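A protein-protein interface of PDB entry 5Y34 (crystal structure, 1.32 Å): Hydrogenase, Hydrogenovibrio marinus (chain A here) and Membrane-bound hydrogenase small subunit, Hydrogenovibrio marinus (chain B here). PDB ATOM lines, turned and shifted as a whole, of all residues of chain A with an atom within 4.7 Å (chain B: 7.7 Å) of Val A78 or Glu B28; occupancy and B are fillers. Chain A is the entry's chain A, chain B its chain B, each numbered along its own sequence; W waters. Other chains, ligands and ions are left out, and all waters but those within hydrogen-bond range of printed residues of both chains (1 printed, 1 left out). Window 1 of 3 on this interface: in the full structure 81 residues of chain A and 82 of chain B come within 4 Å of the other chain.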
ATOM      1  N   GLU A  28      -0.749  19.481 -25.366  1.00  0.00           N
ATOM      2  CA  GLU A  28      -1.254  18.134 -25.237  1.00  0.00           C
ATOM      3  C   GLU A  28      -0.156  17.287 -24.585  1.00  0.00           C
ATOM      4  O   GLU A  28       1.020  17.346 -24.988  1.00  0.00           O
ATOM      5  CB  GLU A  28      -1.623  17.595 -26.611  1.00  0.00           C
ATOM      6  CG  GLU A  28      -2.336  16.249 -26.541  1.00  0.00           C
ATOM      7  CD  GLU A  28      -1.473  15.145 -25.967  1.00  0.00           C
ATOM      8  OE1 GLU A  28      -0.253  15.179 -26.223  1.00  0.00           O
ATOM      9  OE2 GLU A  28      -1.991  14.229 -25.257  1.00  0.00           O
ATOM     10  N   CYS A  76      -3.388  10.393 -30.586  1.00  0.00           N
ATOM     11  CA  CYS A  76      -3.690  11.764 -30.220  1.00  0.00           C
ATOM     12  C   CYS A  76      -5.124  12.142 -30.455  1.00  0.00           C
ATOM     13  O   CYS A  76      -5.649  11.964 -31.554  1.00  0.00           O
ATOM     14  CB  CYS A  76      -2.812  12.712 -30.985  1.00  0.00           C
ATOM     15  SG  CYS A  76      -2.973  14.358 -30.282  1.00  0.00           S
ATOM     16  N   GLY A  77      -5.730  12.731 -29.428  1.00  0.00           N
ATOM     17  CA  GLY A  77      -7.111  13.175 -29.507  1.00  0.00           C
ATOM     18  C   GLY A  77      -7.255  14.639 -29.888  1.00  0.00           C
ATOM     19  O   GLY A  77      -8.366  15.089 -30.103  1.00  0.00           O
ATOM     20  N   VAL A  78      -6.135  15.355 -29.962  1.00  0.00           N
ATOM     21  CA  VAL A  78      -6.122  16.761 -30.374  1.00  0.00           C
ATOM     22  C   VAL A  78      -6.019  16.756 -31.897  1.00  0.00           C
ATOM     23  O   VAL A  78      -6.925  17.227 -32.569  1.00  0.00           O
ATOM     24  CB  VAL A  78      -4.975  17.529 -29.689  1.00  0.00           C
ATOM     25  CG1 VAL A  78      -4.924  18.971 -30.180  1.00  0.00           C
ATOM     26  CG2 VAL A  78      -5.143  17.471 -28.171  1.00  0.00           C
ATOM     27  N   CYS A  79      -4.959  16.150 -32.443  1.00  0.00           N
ATOM     28  CA  CYS A  79      -4.858  15.984 -33.892  1.00  0.00           C
ATOM     29  C   CYS A  79      -5.605  14.707 -34.318  1.00  0.00           C
ATOM     30  O   CYS A  79      -5.068  13.842 -35.003  1.00  0.00           O
ATOM     31  CB  CYS A  79      -3.399  15.993 -34.380  1.00  0.00           C
ATOM     32  SG  CYS A  79      -2.314  14.742 -33.678  1.00  0.00           S
ATOM     33  N   THR A  80      -6.872  14.645 -33.933  1.00  0.00           N
ATOM     34  CA  THR A  80      -7.658  13.449 -34.064  1.00  0.00           C
ATOM     35  C   THR A  80      -8.031  13.189 -35.513  1.00  0.00           C
ATOM     36  O   THR A  80      -8.646  14.023 -36.162  1.00  0.00           O
ATOM     37  CB  THR A  80      -8.893  13.492 -33.162  1.00  0.00           C
ATOM     38  OG1 THR A  80      -9.586  12.268 -33.348  1.00  0.00           O
ATOM     39  CG2 THR A  80      -9.850  14.640 -33.493  1.00  0.00           C
ATOM     40  N   LEU A 114     -10.060  19.200 -39.463  1.00  0.00           N
ATOM     41  CA  LEU A 114      -9.143  19.065 -38.336  1.00  0.00           C
ATOM     42  C   LEU A 114      -8.173  20.267 -38.261  1.00  0.00           C
ATOM     43  O   LEU A 114      -7.941  20.813 -37.163  1.00  0.00           O
ATOM     44  CB  LEU A 114      -8.358  17.751 -38.417  1.00  0.00           C
ATOM     45  CG  LEU A 114      -7.307  17.599 -37.312  1.00  0.00           C
ATOM     46  CD1 LEU A 114      -7.962  17.573 -35.936  1.00  0.00           C
ATOM     47  CD2 LEU A 114      -6.448  16.360 -37.523  1.00  0.00           C
ATOM     48  N   HIS A 117     -10.144  23.337 -36.854  1.00  0.00           N
ATOM     49  CA  HIS A 117     -10.487  23.150 -35.465  1.00  0.00           C
ATOM     50  C   HIS A 117      -9.248  23.204 -34.569  1.00  0.00           C
ATOM     51  O   HIS A 117      -9.216  23.933 -33.535  1.00  0.00           O
ATOM     52  CB  HIS A 117     -11.170  21.776 -35.251  1.00  0.00           C
ATOM     53  CG  HIS A 117     -11.513  21.560 -33.824  1.00  0.00           C
ATOM     54  ND1 HIS A 117     -10.661  20.929 -32.936  1.00  0.00           N
ATOM     55  CD2 HIS A 117     -12.581  21.970 -33.102  1.00  0.00           C
ATOM     56  CE1 HIS A 117     -11.190  20.977 -31.729  1.00  0.00           C
ATOM     57  NE2 HIS A 117     -12.360  21.589 -31.803  1.00  0.00           N
ATOM     58  N   ASP A 118      -8.215  22.453 -34.960  1.00  0.00           N
ATOM     59  CA  ASP A 118      -6.990  22.326 -34.171  1.00  0.00           C
ATOM     60  C   ASP A 118      -6.310  23.713 -34.082  1.00  0.00           C
ATOM     61  O   ASP A 118      -5.923  24.145 -32.987  1.00  0.00           O
ATOM     62  CB  ASP A 118      -6.080  21.265 -34.833  1.00  0.00           C
ATOM     63  CG  ASP A 118      -5.076  20.653 -33.893  1.00  0.00           C
ATOM     64  OD1 ASP A 118      -4.615  21.343 -32.964  1.00  0.00           O
ATOM     65  OD2 ASP A 118      -4.706  19.465 -34.105  1.00  0.00           O
ATOM     66  N   PRO A 229     -14.137  13.666 -30.892  1.00  0.00           N
ATOM     67  CA  PRO A 229     -12.905  13.073 -31.434  1.00  0.00           C
ATOM     68  C   PRO A 229     -13.048  11.645 -31.962  1.00  0.00           C
ATOM     69  O   PRO A 229     -14.015  10.948 -31.658  1.00  0.00           O
ATOM     70  CB  PRO A 229     -11.972  13.035 -30.206  1.00  0.00           C
ATOM     71  CG  PRO A 229     -12.444  14.196 -29.361  1.00  0.00           C
ATOM     72  CD  PRO A 229     -13.937  14.197 -29.526  1.00  0.00           C
ATOM     73  N   ARG A 523       0.509  20.000 -37.050  1.00  0.00           N
ATOM     74  CA  ARG A 523       1.782  20.470 -36.473  1.00  0.00           C
ATOM     75  C   ARG A 523       2.990  20.268 -37.381  1.00  0.00           C
ATOM     76  O   ARG A 523       4.121  20.572 -36.989  1.00  0.00           O
ATOM     77  CB  ARG A 523       2.016  19.832 -35.105  1.00  0.00           C
ATOM     78  CG  ARG A 523       1.040  20.358 -34.086  1.00  0.00           C
ATOM     79  CD  ARG A 523       0.798  19.395 -32.942  1.00  0.00           C
ATOM     80  NE  ARG A 523      -0.268  19.887 -32.083  1.00  0.00           N
ATOM     81  CZ  ARG A 523      -1.564  19.840 -32.356  1.00  0.00           C
ATOM     82  NH1 ARG A 523      -2.018  19.180 -33.417  1.00  0.00           N
ATOM     83  NH2 ARG A 523      -2.426  20.393 -31.520  1.00  0.00           N
ATOM     84  N   TRP B  17      -8.553  18.027 -12.409  1.00  0.00           N
ATOM     85  CA  TRP B  17      -8.568  17.153 -13.579  1.00  0.00           C
ATOM     86  C   TRP B  17      -7.130  16.754 -13.905  1.00  0.00           C
ATOM     87  O   TRP B  17      -6.360  17.528 -14.466  1.00  0.00           O
ATOM     88  CB  TRP B  17      -9.256  17.867 -14.755  1.00  0.00           C
ATOM     89  CG  TRP B  17      -9.545  17.050 -15.992  1.00  0.00           C
ATOM     90  CD1 TRP B  17      -8.718  16.141 -16.632  1.00  0.00           C
ATOM     91  CD2 TRP B  17     -10.718  17.157 -16.802  1.00  0.00           C
ATOM     92  NE1 TRP B  17      -9.341  15.665 -17.765  1.00  0.00           N
ATOM     93  CE2 TRP B  17     -10.573  16.255 -17.884  1.00  0.00           C
ATOM     94  CE3 TRP B  17     -11.903  17.899 -16.693  1.00  0.00           C
ATOM     95  CZ2 TRP B  17     -11.558  16.111 -18.874  1.00  0.00           C
ATOM     96  CZ3 TRP B  17     -12.885  17.753 -17.679  1.00  0.00           C
ATOM     97  CH2 TRP B  17     -12.708  16.860 -18.744  1.00  0.00           C
ATOM     98  N   HIS B  19      -4.140  14.196 -15.683  1.00  0.00           N
ATOM     99  CA  HIS B  19      -3.885  13.563 -16.975  1.00  0.00           C
ATOM    100  C   HIS B  19      -2.711  12.618 -16.821  1.00  0.00           C
ATOM    101  O   HIS B  19      -1.594  13.036 -16.522  1.00  0.00           O
ATOM    102  CB  HIS B  19      -3.509  14.611 -18.023  1.00  0.00           C
ATOM    103  CG  HIS B  19      -4.614  15.547 -18.365  1.00  0.00           C
ATOM    104  ND1 HIS B  19      -5.471  15.335 -19.421  1.00  0.00           N
ATOM    105  CD2 HIS B  19      -4.992  16.718 -17.800  1.00  0.00           C
ATOM    106  CE1 HIS B  19      -6.329  16.339 -19.499  1.00  0.00           C
ATOM    107  NE2 HIS B  19      -6.062  17.187 -18.521  1.00  0.00           N
ATOM    108  N   GLU B  22      -2.328   9.174 -21.911  1.00  0.00           N
ATOM    109  CA  GLU B  22      -3.573   9.519 -22.543  1.00  0.00           C
ATOM    110  C   GLU B  22      -3.286  10.051 -23.934  1.00  0.00           C
ATOM    111  O   GLU B  22      -2.129  10.278 -24.309  1.00  0.00           O
ATOM    112  CB  GLU B  22      -4.287  10.614 -21.748  1.00  0.00           C
ATOM    113  CG  GLU B  22      -3.549  11.949 -21.797  1.00  0.00           C
ATOM    114  CD  GLU B  22      -4.347  13.076 -21.182  1.00  0.00           C
ATOM    115  OE1 GLU B  22      -5.046  12.827 -20.185  1.00  0.00           O
ATOM    116  OE2 GLU B  22      -4.292  14.205 -21.698  1.00  0.00           O
ATOM    117  N   CYS B  23      -4.362  10.287 -24.673  1.00  0.00           N
ATOM    118  CA  CYS B  23      -4.297  11.004 -25.956  1.00  0.00           C
ATOM    119  C   CYS B  23      -4.999  12.378 -25.897  1.00  0.00           C
ATOM    120  O   CYS B  23      -4.899  13.150 -26.857  1.00  0.00           O
ATOM    121  CB  CYS B  23      -4.856  10.136 -27.107  1.00  0.00           C
ATOM    122  SG  CYS B  23      -6.648  10.286 -27.321  1.00  0.00           S
ATOM    123  N   THR B  24      -5.711  12.640 -24.793  1.00  0.00           N
ATOM    124  CA  THR B  24      -6.437  13.904 -24.543  1.00  0.00           C
ATOM    125  C   THR B  24      -7.811  13.983 -25.226  1.00  0.00           C
ATOM    126  O   THR B  24      -8.479  15.017 -25.209  1.00  0.00           O
ATOM    127  CB  THR B  24      -5.540  15.141 -24.809  1.00  0.00           C
ATOM    128  OG1 THR B  24      -4.235  14.878 -24.269  1.00  0.00           O
ATOM    129  CG2 THR B  24      -6.081  16.403 -24.124  1.00  0.00           C
ATOM    130  N   CYS B  25      -8.269  12.856 -25.774  1.00  0.00           N
ATOM    131  CA  CYS B  25      -9.558  12.874 -26.471  1.00  0.00           C
ATOM    132  C   CYS B  25     -10.719  13.171 -25.522  1.00  0.00           C
ATOM    133  O   CYS B  25     -11.683  13.823 -25.938  1.00  0.00           O
ATOM    134  CB  CYS B  25      -9.822  11.530 -27.202  1.00  0.00           C
ATOM    135  SG  CYS B  25      -9.968  10.032 -26.171  1.00  0.00           S
ATOM    136  N   CYS B  26     -10.660  12.683 -24.271  1.00  0.00           N
ATOM    137  CA  CYS B  26     -11.762  12.973 -23.351  1.00  0.00           C
ATOM    138  C   CYS B  26     -11.889  14.467 -23.048  1.00  0.00           C
ATOM    139  O   CYS B  26     -12.999  14.986 -22.978  1.00  0.00           O
ATOM    140  CB  CYS B  26     -11.637  12.156 -22.059  1.00  0.00           C
ATOM    141  SG  CYS B  26     -11.215  10.416 -22.343  1.00  0.00           S
ATOM    142  N   SER B  27     -10.754  15.130 -22.849  1.00  0.00           N
ATOM    143  CA  SER B  27     -10.752  16.585 -22.652  1.00  0.00           C
ATOM    144  C   SER B  27     -11.346  17.322 -23.852  1.00  0.00           C
ATOM    145  O   SER B  27     -12.146  18.263 -23.689  1.00  0.00           O
ATOM    146  CB  SER B  27      -9.327  17.049 -22.439  1.00  0.00           C
ATOM    147  OG  SER B  27      -8.923  16.815 -21.121  1.00  0.00           O
ATOM    148  N   GLU B  28     -10.928  16.897 -25.042  1.00  0.00           N
ATOM    149  CA  GLU B  28     -11.509  17.415 -26.267  1.00  0.00           C
ATOM    150  C   GLU B  28     -12.997  17.164 -26.361  1.00  0.00           C
ATOM    151  O   GLU B  28     -13.778  18.053 -26.697  1.00  0.00           O
ATOM    152  CB  GLU B  28     -10.767  16.902 -27.490  1.00  0.00           C
ATOM    153  CG  GLU B  28      -9.340  17.425 -27.618  1.00  0.00           C
ATOM    154  CD  GLU B  28      -9.246  18.793 -28.252  1.00  0.00           C
ATOM    155  OE1 GLU B  28     -10.273  19.379 -28.681  1.00  0.00           O
ATOM    156  OE2 GLU B  28      -8.098  19.264 -28.348  1.00  0.00           O
ATOM    157  N   SER B  29     -13.412  15.920 -26.062  1.00  0.00           N
ATOM    158  CA  SER B  29     -14.831  15.683 -26.101  1.00  0.00           C
ATOM    159  C   SER B  29     -15.616  16.592 -25.169  1.00  0.00           C
ATOM    160  O   SER B  29     -16.652  17.123 -25.548  1.00  0.00           O
ATOM    161  CB  SER B  29     -15.121  14.217 -25.776  1.00  0.00           C
ATOM    162  OG  SER B  29     -16.458  13.947 -26.170  1.00  0.00           O
ATOM    163  N   PHE B  30     -15.100  16.780 -23.955  1.00  0.00           N
ATOM    164  CA  PHE B  30     -15.782  17.599 -22.971  1.00  0.00           C
ATOM    165  C   PHE B  30     -16.147  18.976 -23.534  1.00  0.00           C
ATOM    166  O   PHE B  30     -17.268  19.438 -23.349  1.00  0.00           O
ATOM    167  CB  PHE B  30     -14.882  17.735 -21.744  1.00  0.00           C
ATOM    168  CG  PHE B  30     -15.572  18.306 -20.541  1.00  0.00           C
ATOM    169  CD1 PHE B  30     -16.308  17.462 -19.710  1.00  0.00           C
ATOM    170  CD2 PHE B  30     -15.476  19.650 -20.231  1.00  0.00           C
ATOM    171  CE1 PHE B  30     -16.950  17.942 -18.591  1.00  0.00           C
ATOM    172  CE2 PHE B  30     -16.119  20.155 -19.091  1.00  0.00           C
ATOM    173  CZ  PHE B  30     -16.856  19.295 -18.281  1.00  0.00           C
ATOM    174  N   ILE B  31     -15.220  19.592 -24.258  1.00  0.00           N
ATOM    175  CA  ILE B  31     -15.488  20.946 -24.742  1.00  0.00           C
ATOM    176  C   ILE B  31     -16.397  20.971 -25.963  1.00  0.00           C
ATOM    177  O   ILE B  31     -16.825  22.038 -26.390  1.00  0.00           O
ATOM    178  CB  ILE B  31     -14.214  21.773 -24.979  1.00  0.00           C
ATOM    179  CG1 ILE B  31     -13.388  21.250 -26.177  1.00  0.00           C
ATOM    180  CG2 ILE B  31     -13.442  21.883 -23.669  1.00  0.00           C
ATOM    181  CD1 ILE B  31     -12.323  22.231 -26.651  1.00  0.00           C
ATOM    182  N   ARG B  32     -16.746  19.789 -26.494  1.00  0.00           N
ATOM    183  CA  ARG B  32     -17.747  19.718 -27.560  1.00  0.00           C
ATOM    184  C   ARG B  32     -19.172  19.835 -27.035  1.00  0.00           C
ATOM    185  O   ARG B  32     -20.103  19.929 -27.830  1.00  0.00           O
ATOM    186  CB  ARG B  32     -17.627  18.419 -28.372  1.00  0.00           C
ATOM    187  CG  ARG B  32     -16.266  18.145 -28.968  1.00  0.00           C
ATOM    188  CD  ARG B  32     -15.753  19.205 -29.953  1.00  0.00           C
ATOM    189  NE  ARG B  32     -14.587  18.609 -30.567  1.00  0.00           N
ATOM    190  CZ  ARG B  32     -13.340  18.726 -30.145  1.00  0.00           C
ATOM    191  NH1 ARG B  32     -13.022  19.686 -29.247  1.00  0.00           N
ATOM    192  NH2 ARG B  32     -12.386  18.009 -30.718  1.00  0.00           N
ATOM    193  N   SER B  33     -19.354  19.819 -25.715  1.00  0.00           N
ATOM    194  CA  SER B  33     -20.688  19.759 -25.161  1.00  0.00           C
ATOM    195  C   SER B  33     -21.614  20.846 -25.683  1.00  0.00           C
ATOM    196  O   SER B  33     -21.293  22.052 -25.608  1.00  0.00           O
ATOM    197  CB  SER B  33     -20.667  19.785 -23.644  1.00  0.00           C
ATOM    198  OG  SER B  33     -21.990  19.706 -23.131  1.00  0.00           O
ATOM    199  N   ALA B  38     -19.254  24.187 -22.427  1.00  0.00           N
ATOM    200  CA  ALA B  38     -18.069  24.075 -21.567  1.00  0.00           C
ATOM    201  C   ALA B  38     -17.727  25.404 -20.886  1.00  0.00           C
ATOM    202  O   ALA B  38     -17.364  25.444 -19.712  1.00  0.00           O
ATOM    203  CB  ALA B  38     -16.875  23.567 -22.358  1.00  0.00           C
ATOM    204  N   THR B  53      -4.047  20.968 -19.290  1.00  0.00           N
ATOM    205  CA  THR B  53      -4.427  21.349 -20.666  1.00  0.00           C
ATOM    206  C   THR B  53      -4.738  22.835 -20.873  1.00  0.00           C
ATOM    207  O   THR B  53      -4.341  23.430 -21.878  1.00  0.00           O
ATOM    208  CB  THR B  53      -5.674  20.568 -21.136  1.00  0.00           C
ATOM    209  OG1 THR B  53      -5.469  19.168 -20.932  1.00  0.00           O
ATOM    210  CG2 THR B  53      -5.959  20.807 -22.618  1.00  0.00           C
ATOM    211  N   GLU B  82      -8.227  11.673 -16.435  1.00  0.00           N
ATOM    212  CA  GLU B  82      -8.137  11.201 -17.814  1.00  0.00           C
ATOM    213  C   GLU B  82      -6.794  10.495 -17.950  1.00  0.00           C
ATOM    214  O   GLU B  82      -5.811  10.876 -17.325  1.00  0.00           O
ATOM    215  CB  GLU B  82      -8.255  12.368 -18.805  1.00  0.00           C
ATOM    216  CG  GLU B  82      -8.319  11.929 -20.261  1.00  0.00           C
ATOM    217  CD  GLU B  82      -8.404  13.097 -21.221  1.00  0.00           C
ATOM    218  OE1 GLU B  82      -8.260  14.246 -20.758  1.00  0.00           O
ATOM    219  OE2 GLU B  82      -8.613  12.871 -22.435  1.00  0.00           O
ATOM    220  N   PRO B 159     -13.377   8.841 -27.124  1.00  0.00           N
ATOM    221  CA  PRO B 159     -13.719   9.271 -25.793  1.00  0.00           C
ATOM    222  C   PRO B 159     -15.197   9.020 -25.480  1.00  0.00           C
ATOM    223  O   PRO B 159     -15.938   8.549 -26.351  1.00  0.00           O
ATOM    224  CB  PRO B 159     -13.481  10.787 -25.886  1.00  0.00           C
ATOM    225  CG  PRO B 159     -13.869  11.145 -27.308  1.00  0.00           C
ATOM    226  CD  PRO B 159     -13.634   9.885 -28.133  1.00  0.00           C
ATOM    227  N   PRO B 160     -15.646   9.365 -24.266  1.00  0.00           N
ATOM    228  CA  PRO B 160     -17.083   9.398 -24.022  1.00  0.00           C
ATOM    229  C   PRO B 160     -17.760  10.515 -24.827  1.00  0.00           C
ATOM    230  O   PRO B 160     -17.103  11.511 -25.222  1.00  0.00           O
ATOM    231  CB  PRO B 160     -17.192   9.709 -22.522  1.00  0.00           C
ATOM    232  CG  PRO B 160     -15.822   9.537 -21.963  1.00  0.00           C
ATOM    233  CD  PRO B 160     -14.878   9.792 -23.088  1.00  0.00           C
ATOM    234  N   ALA B 162     -19.738  13.884 -25.460  1.00  0.00           N
ATOM    235  CA  ALA B 162     -19.577  15.150 -24.742  1.00  0.00           C
ATOM    236  C   ALA B 162     -20.689  15.396 -23.737  1.00  0.00           C
ATOM    237  O   ALA B 162     -20.417  15.757 -22.570  1.00  0.00           O
ATOM    238  CB  ALA B 162     -19.509  16.301 -25.737  1.00  0.00           C
ATOM    239  N   MET B 165     -20.500  13.325 -20.618  1.00  0.00           N
ATOM    240  CA  MET B 165     -19.555  13.889 -19.643  1.00  0.00           C
ATOM    241  C   MET B 165     -20.149  15.057 -18.856  1.00  0.00           C
ATOM    242  O   MET B 165     -20.154  15.072 -17.624  1.00  0.00           O
ATOM    243  CB  MET B 165     -18.270  14.335 -20.342  1.00  0.00           C
ATOM    244  CG  MET B 165     -17.528  13.217 -21.049  1.00  0.00           C
ATOM    245  SD  MET B 165     -16.034  13.773 -21.900  1.00  0.00           S
ATOM    246  CE  MET B 165     -14.883  13.872 -20.521  1.00  0.00           C
ATOM    247  N   ASN B 245     -21.726  14.760 -30.955  1.00  0.00           N
ATOM    248  CA  ASN B 245     -21.501  16.119 -31.518  1.00  0.00           C
ATOM    249  C   ASN B 245     -22.812  16.874 -31.699  1.00  0.00           C
ATOM    250  O   ASN B 245     -23.202  17.258 -32.803  1.00  0.00           O
ATOM    251  CB  ASN B 245     -20.674  16.027 -32.802  1.00  0.00           C
ATOM    252  CG  ASN B 245     -19.329  15.396 -32.566  1.00  0.00           C
ATOM    253  OD1 ASN B 245     -19.131  14.212 -32.897  1.00  0.00           O
ATOM    254  ND2 ASN B 245     -18.417  16.118 -31.930  1.00  0.00           N
HETATM  255  O   HOH W   1     -10.913  17.787 -33.638  1.00  0.00           O
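Of the 22 printed residues of chain B, 7 touch a printed residue of chain A. Hydrophobic or aromatic side chains of chain B that line the printed part of chain A: Pro B159. Hydrophobic or aromatic side chains of chain A that line the printed part of chain B: Val A78, His A117 and Pro A229. Among the printed residues, no Asp or Glu carboxylate lies within 4 Å of a Lys or Arg side-chain nitrogen of the other chain.
Water W1 lies within hydrogen-bond range of ND1 of His A117 (3.2 Å) and NH2 of Arg B32 (3.3 Å).
The side-chain sulfur (SG) of Cys A76 sits close to the backbone NH (N) of Val A78, 3.3 Å away. The side-chain carboxylate (OE2) of Glu B22 sits at hydrogen-bond distance from the side-chain hydroxyl (OG1) of Thr B24, at 2.7 Å. The backbone NH of Cys B25 lies within hydrogen-bond range of the side-chain carboxylate of Glu B82, at 3.4 Å. OE1 of Glu B28 is in salt-bridge range of NH1 of Arg B32 (2.8 Å). O of Pro B160 is in hydrogen-bond range of OG of Ser B29 (2.7 Å). OG of Ser B29 lies within hydrogen-bond range of N of Ala B162 (3.4 Å).
Among the printed residues, merely in contact across the chains: Val A78 with Glu B28, Pro A229 with Cys B25, Gly A77 with Glu B28, His A117 with Glu B28, Pro A229 with Glu B28, Cys A76 with Cys B23, Pro A229 with Pro B159, Pro A229 with Ser B29 and Gly A77 with Cys B25.
Printed residues of chain B within 4 Å of Cys A76: Cys B23. Of chain B, only Cys B23, Cys B25 and Glu B28 come within 4 Å of Gly A77. Thr A80 touches none of the printed residues of chain B. Leu A114 touches none of the printed residues of chain B. Printed residues of chain B within 4 Å of Pro A229: Cys B25, Glu B28, Ser B29 and Pro B159. Of the printed residues of chain A, Cys B25 touches Gly A77 (3.9 Å) and Pro A229 (3.5 Å). Of chain A, only Gly A77, Val A78, His A117 and Pro A229 come within 4 Å of Glu B28. Printed residues of chain A within 4 Å of Ser B29: Pro A229. Of the printed residues of chain A, Pro B159 touches Pro A229 (3.7 Å). The nearest printed residue of chain A that does not touch Glu B28 is Cys A79 (6.0 Å). The nearest printed residue of chain A that does not touch Thr B24 is Val A78 (4.1 Å).
OG1 of Thr B24 sits at hydrogen-bond distance from OE2 of Glu A28 (2.5 Å). O of Cys B23 lies within hydrogen-bond range of N of Gly A77, at 2.7 Å. A ring nitrogen (NE2) of His A117 sits at hydrogen-bond distance from the guanidinium group of Arg B32. The side-chain carboxylate of Glu A28 lies close to the backbone carbonyl oxygen of Cys B23.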
